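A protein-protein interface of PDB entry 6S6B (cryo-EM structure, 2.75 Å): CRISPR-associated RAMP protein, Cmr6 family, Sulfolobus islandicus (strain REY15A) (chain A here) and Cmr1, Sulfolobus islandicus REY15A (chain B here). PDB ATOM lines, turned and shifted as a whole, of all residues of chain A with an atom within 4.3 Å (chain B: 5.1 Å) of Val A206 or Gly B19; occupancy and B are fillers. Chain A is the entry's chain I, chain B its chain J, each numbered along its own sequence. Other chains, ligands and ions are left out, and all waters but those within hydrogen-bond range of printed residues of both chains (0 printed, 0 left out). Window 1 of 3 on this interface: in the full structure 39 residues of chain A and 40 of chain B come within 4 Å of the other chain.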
ATOM      1  N   ASP A 205     -16.516  22.626  -8.471  1.00  0.00           N
ATOM      2  CA  ASP A 205     -16.247  23.979  -8.020  1.00  0.00           C
ATOM      3  C   ASP A 205     -17.129  24.259  -6.818  1.00  0.00           C
ATOM      4  O   ASP A 205     -17.889  23.399  -6.371  1.00  0.00           O
ATOM      5  CB  ASP A 205     -16.478  24.995  -9.134  1.00  0.00           C
ATOM      6  CG  ASP A 205     -15.529  26.164  -9.050  1.00  0.00           C
ATOM      7  OD1 ASP A 205     -15.263  26.623  -7.924  1.00  0.00           O
ATOM      8  OD2 ASP A 205     -15.042  26.622 -10.103  1.00  0.00           O
ATOM      9  N   VAL A 206     -17.023  25.474  -6.292  1.00  0.00           N
ATOM     10  CA  VAL A 206     -17.764  25.850  -5.099  1.00  0.00           C
ATOM     11  C   VAL A 206     -18.098  27.331  -5.172  1.00  0.00           C
ATOM     12  O   VAL A 206     -17.368  28.128  -5.764  1.00  0.00           O
ATOM     13  CB  VAL A 206     -16.971  25.512  -3.816  1.00  0.00           C
ATOM     14  CG1 VAL A 206     -15.816  26.464  -3.640  1.00  0.00           C
ATOM     15  CG2 VAL A 206     -17.875  25.546  -2.609  1.00  0.00           C
ATOM     16  N   ILE A 207     -19.240  27.686  -4.594  1.00  0.00           N
ATOM     17  CA  ILE A 207     -19.636  29.066  -4.363  1.00  0.00           C
ATOM     18  C   ILE A 207     -20.107  29.138  -2.925  1.00  0.00           C
ATOM     19  O   ILE A 207     -21.056  28.442  -2.548  1.00  0.00           O
ATOM     20  CB  ILE A 207     -20.748  29.525  -5.318  1.00  0.00           C
ATOM     21  CG1 ILE A 207     -20.198  29.727  -6.726  1.00  0.00           C
ATOM     22  CG2 ILE A 207     -21.378  30.802  -4.818  1.00  0.00           C
ATOM     23  CD1 ILE A 207     -19.443  31.020  -6.904  1.00  0.00           C
ATOM     24  N   THR A 208     -19.441  29.956  -2.115  1.00  0.00           N
ATOM     25  CA  THR A 208     -19.715  30.042  -0.685  1.00  0.00           C
ATOM     26  C   THR A 208     -20.102  31.471  -0.337  1.00  0.00           C
ATOM     27  O   THR A 208     -19.255  32.265   0.092  1.00  0.00           O
ATOM     28  CB  THR A 208     -18.509  29.603   0.137  1.00  0.00           C
ATOM     29  OG1 THR A 208     -18.004  28.372  -0.385  1.00  0.00           O
ATOM     30  CG2 THR A 208     -18.906  29.392   1.569  1.00  0.00           C
ATOM     31  N   VAL A 225     -21.666  25.698  -1.749  1.00  0.00           N
ATOM     32  CA  VAL A 225     -22.469  25.116  -2.822  1.00  0.00           C
ATOM     33  C   VAL A 225     -21.497  24.447  -3.788  1.00  0.00           C
ATOM     34  O   VAL A 225     -20.941  25.092  -4.682  1.00  0.00           O
ATOM     35  CB  VAL A 225     -23.335  26.156  -3.537  1.00  0.00           C
ATOM     36  CG1 VAL A 225     -24.076  25.529  -4.698  1.00  0.00           C
ATOM     37  CG2 VAL A 225     -24.308  26.776  -2.568  1.00  0.00           C
ATOM     38  N   ILE A 226     -21.281  23.144  -3.615  1.00  0.00           N
ATOM     39  CA  ILE A 226     -20.535  22.379  -4.602  1.00  0.00           C
ATOM     40  C   ILE A 226     -21.364  22.265  -5.873  1.00  0.00           C
ATOM     41  O   ILE A 226     -22.595  22.166  -5.831  1.00  0.00           O
ATOM     42  CB  ILE A 226     -20.170  20.987  -4.056  1.00  0.00           C
ATOM     43  CG1 ILE A 226     -19.645  21.093  -2.630  1.00  0.00           C
ATOM     44  CG2 ILE A 226     -19.140  20.321  -4.936  1.00  0.00           C
ATOM     45  CD1 ILE A 226     -18.275  21.693  -2.540  1.00  0.00           C
ATOM     46  N   HIS A 227     -20.693  22.277  -7.015  1.00  0.00           N
ATOM     47  CA  HIS A 227     -21.379  22.122  -8.286  1.00  0.00           C
ATOM     48  C   HIS A 227     -20.359  21.700  -9.332  1.00  0.00           C
ATOM     49  O   HIS A 227     -19.174  21.536  -9.041  1.00  0.00           O
ATOM     50  CB  HIS A 227     -22.095  23.411  -8.685  1.00  0.00           C
ATOM     51  CG  HIS A 227     -21.186  24.582  -8.853  1.00  0.00           C
ATOM     52  ND1 HIS A 227     -20.848  25.414  -7.811  1.00  0.00           N
ATOM     53  CD2 HIS A 227     -20.559  25.072  -9.947  1.00  0.00           C
ATOM     54  CE1 HIS A 227     -20.043  26.363  -8.254  1.00  0.00           C
ATOM     55  NE2 HIS A 227     -19.850  26.176  -9.546  1.00  0.00           N
ATOM     56  N   THR B  17      -5.911  30.342  -0.217  1.00  0.00           N
ATOM     57  CA  THR B  17      -7.095  30.247  -1.055  1.00  0.00           C
ATOM     58  C   THR B  17      -7.645  28.830  -1.046  1.00  0.00           C
ATOM     59  O   THR B  17      -6.892  27.857  -1.113  1.00  0.00           O
ATOM     60  CB  THR B  17      -6.750  30.665  -2.483  1.00  0.00           C
ATOM     61  OG1 THR B  17      -6.280  32.016  -2.486  1.00  0.00           O
ATOM     62  CG2 THR B  17      -7.961  30.566  -3.372  1.00  0.00           C
ATOM     63  N   GLY B  18      -8.968  28.718  -0.953  1.00  0.00           N
ATOM     64  CA  GLY B  18      -9.631  27.439  -0.870  1.00  0.00           C
ATOM     65  C   GLY B  18     -10.230  27.000  -2.193  1.00  0.00           C
ATOM     66  O   GLY B  18      -9.931  27.530  -3.263  1.00  0.00           O
ATOM     67  N   GLY B  19     -11.091  26.002  -2.103  1.00  0.00           N
ATOM     68  CA  GLY B  19     -11.738  25.462  -3.274  1.00  0.00           C
ATOM     69  C   GLY B  19     -12.859  24.553  -2.850  1.00  0.00           C
ATOM     70  O   GLY B  19     -13.360  24.648  -1.732  1.00  0.00           O
ATOM     71  N   TYR B  20     -13.249  23.656  -3.753  1.00  0.00           N
ATOM     72  CA  TYR B  20     -14.317  22.726  -3.409  1.00  0.00           C
ATOM     73  C   TYR B  20     -13.886  21.774  -2.303  1.00  0.00           C
ATOM     74  O   TYR B  20     -14.728  21.285  -1.545  1.00  0.00           O
ATOM     75  CB  TYR B  20     -14.773  21.961  -4.650  1.00  0.00           C
ATOM     76  CG  TYR B  20     -13.913  20.788  -5.040  1.00  0.00           C
ATOM     77  CD1 TYR B  20     -14.097  19.542  -4.461  1.00  0.00           C
ATOM     78  CD2 TYR B  20     -12.933  20.919  -6.004  1.00  0.00           C
ATOM     79  CE1 TYR B  20     -13.320  18.478  -4.814  1.00  0.00           C
ATOM     80  CE2 TYR B  20     -12.154  19.853  -6.367  1.00  0.00           C
ATOM     81  CZ  TYR B  20     -12.350  18.635  -5.767  1.00  0.00           C
ATOM     82  OH  TYR B  20     -11.572  17.560  -6.122  1.00  0.00           O
ATOM     83  N   ASN B  21     -12.587  21.505  -2.192  1.00  0.00           N
ATOM     84  CA  ASN B  21     -12.047  20.649  -1.149  1.00  0.00           C
ATOM     85  C   ASN B  21     -11.427  21.447  -0.016  1.00  0.00           C
ATOM     86  O   ASN B  21     -10.781  20.864   0.860  1.00  0.00           O
ATOM     87  CB  ASN B  21     -11.013  19.694  -1.735  1.00  0.00           C
ATOM     88  CG  ASN B  21      -9.926  20.415  -2.481  1.00  0.00           C
ATOM     89  OD1 ASN B  21     -10.025  21.612  -2.734  1.00  0.00           O
ATOM     90  ND2 ASN B  21      -8.878  19.695  -2.841  1.00  0.00           N
ATOM     91  N   ARG B  22     -11.595  22.767  -0.030  1.00  0.00           N
ATOM     92  CA  ARG B  22     -11.052  23.707   0.942  1.00  0.00           C
ATOM     93  C   ARG B  22      -9.540  23.850   0.846  1.00  0.00           C
ATOM     94  O   ARG B  22      -8.910  24.285   1.811  1.00  0.00           O
ATOM     95  CB  ARG B  22     -11.445  23.337   2.376  1.00  0.00           C
ATOM     96  CG  ARG B  22     -12.796  23.878   2.782  1.00  0.00           C
ATOM     97  CD  ARG B  22     -13.075  23.647   4.246  1.00  0.00           C
ATOM     98  NE  ARG B  22     -13.475  22.270   4.496  1.00  0.00           N
ATOM     99  CZ  ARG B  22     -14.386  21.907   5.391  1.00  0.00           C
ATOM    100  NH1 ARG B  22     -14.996  22.823   6.127  1.00  0.00           N
ATOM    101  NH2 ARG B  22     -14.687  20.627   5.548  1.00  0.00           N
ATOM    102  N   HIS B  23      -8.942  23.505  -0.288  1.00  0.00           N
ATOM    103  CA  HIS B  23      -7.514  23.675  -0.515  1.00  0.00           C
ATOM    104  C   HIS B  23      -7.288  24.398  -1.833  1.00  0.00           C
ATOM    105  O   HIS B  23      -8.180  24.499  -2.675  1.00  0.00           O
ATOM    106  CB  HIS B  23      -6.785  22.329  -0.522  1.00  0.00           C
ATOM    107  CG  HIS B  23      -6.911  21.572   0.759  1.00  0.00           C
ATOM    108  ND1 HIS B  23      -7.293  20.252   0.807  1.00  0.00           N
ATOM    109  CD2 HIS B  23      -6.711  21.954   2.041  1.00  0.00           C
ATOM    110  CE1 HIS B  23      -7.323  19.850   2.064  1.00  0.00           C
ATOM    111  NE2 HIS B  23      -6.971  20.864   2.833  1.00  0.00           N
ATOM    112  N   ARG B  34      -8.711  33.130  -6.244  1.00  0.00           N
ATOM    113  CA  ARG B  34     -10.061  32.977  -6.759  1.00  0.00           C
ATOM    114  C   ARG B  34     -10.635  34.345  -7.077  1.00  0.00           C
ATOM    115  O   ARG B  34     -10.846  35.142  -6.154  1.00  0.00           O
ATOM    116  CB  ARG B  34     -10.944  32.250  -5.751  1.00  0.00           C
ATOM    117  CG  ARG B  34     -10.671  30.771  -5.669  1.00  0.00           C
ATOM    118  CD  ARG B  34     -11.402  30.121  -4.517  1.00  0.00           C
ATOM    119  NE  ARG B  34     -12.841  30.048  -4.739  1.00  0.00           N
ATOM    120  CZ  ARG B  34     -13.429  29.231  -5.605  1.00  0.00           C
ATOM    121  NH1 ARG B  34     -12.707  28.406  -6.347  1.00  0.00           N
ATOM    122  NH2 ARG B  34     -14.746  29.240  -5.729  1.00  0.00           N
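Of the 7 printed residues of chain A, 3 touch a printed residue of chain B. Hydrophobic or aromatic side chains of chain A within 4 Å of the printed part of chain B: Val A206 and Ile A226. Printed residues of chain B that touch a printed residue of chain A: Gly B19, Tyr B20 and Arg B34. Hydrophobic or aromatic side chains of chain B that line the printed part of chain A: Tyr B20. Among the printed residues, Asp or Glu carboxylates within 4 Å of a Lys or Arg side-chain nitrogen of the other chain: Asp A205 with Arg B34 (3.5 Å).
Asp A205 touches Tyr B20 (O to CB, 3.8 Å). Val A206 touches Gly B19. CG1 of Val A206 touches N of Tyr B20 (3.8 Å). Tyr B20 touches Ile A226.
Of the printed residues of chain B, Asp A205 touches Tyr B20 (3.8 Å) and Arg B34 (3.5 Å). Of chain B, only Gly B19 (3.6 Å), Tyr B20 (3.8 Å) and Arg B34 (2.8 Å) come within 4 Å of Val A206. Ile A207 touches none of the printed residues of chain B. Printed residues of chain B within 4 Å of Ile A226: Tyr B20 (3.7 Å). Printed residues of chain A within 4 Å of Gly B19: Val A206 (3.6 Å). Printed residues of chain A within 4 Å of Tyr B20: Asp A205, Val A206 and Ile A226. Printed residues of chain A within 4 Å of Arg B34: Asp A205 and Val A206. The nearest printed residue of chain B that does not touch Val A206 is Gly B18 (5.8 Å).
The backbone NH (N) of Asp A205 lies within hydrogen-bond range of the backbone carbonyl oxygen (O) of His A227 (2.9 Å).
The backbone carbonyl oxygen (O) of Val A206 lies within hydrogen-bond range of the guanidinium group (NH2) of Arg B34, 2.8 Å away. The guanidinium group (NH2) of Arg B34 is in salt-bridge range of the side-chain carboxylate (OD1) of Asp A205, 3.5 Å away.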
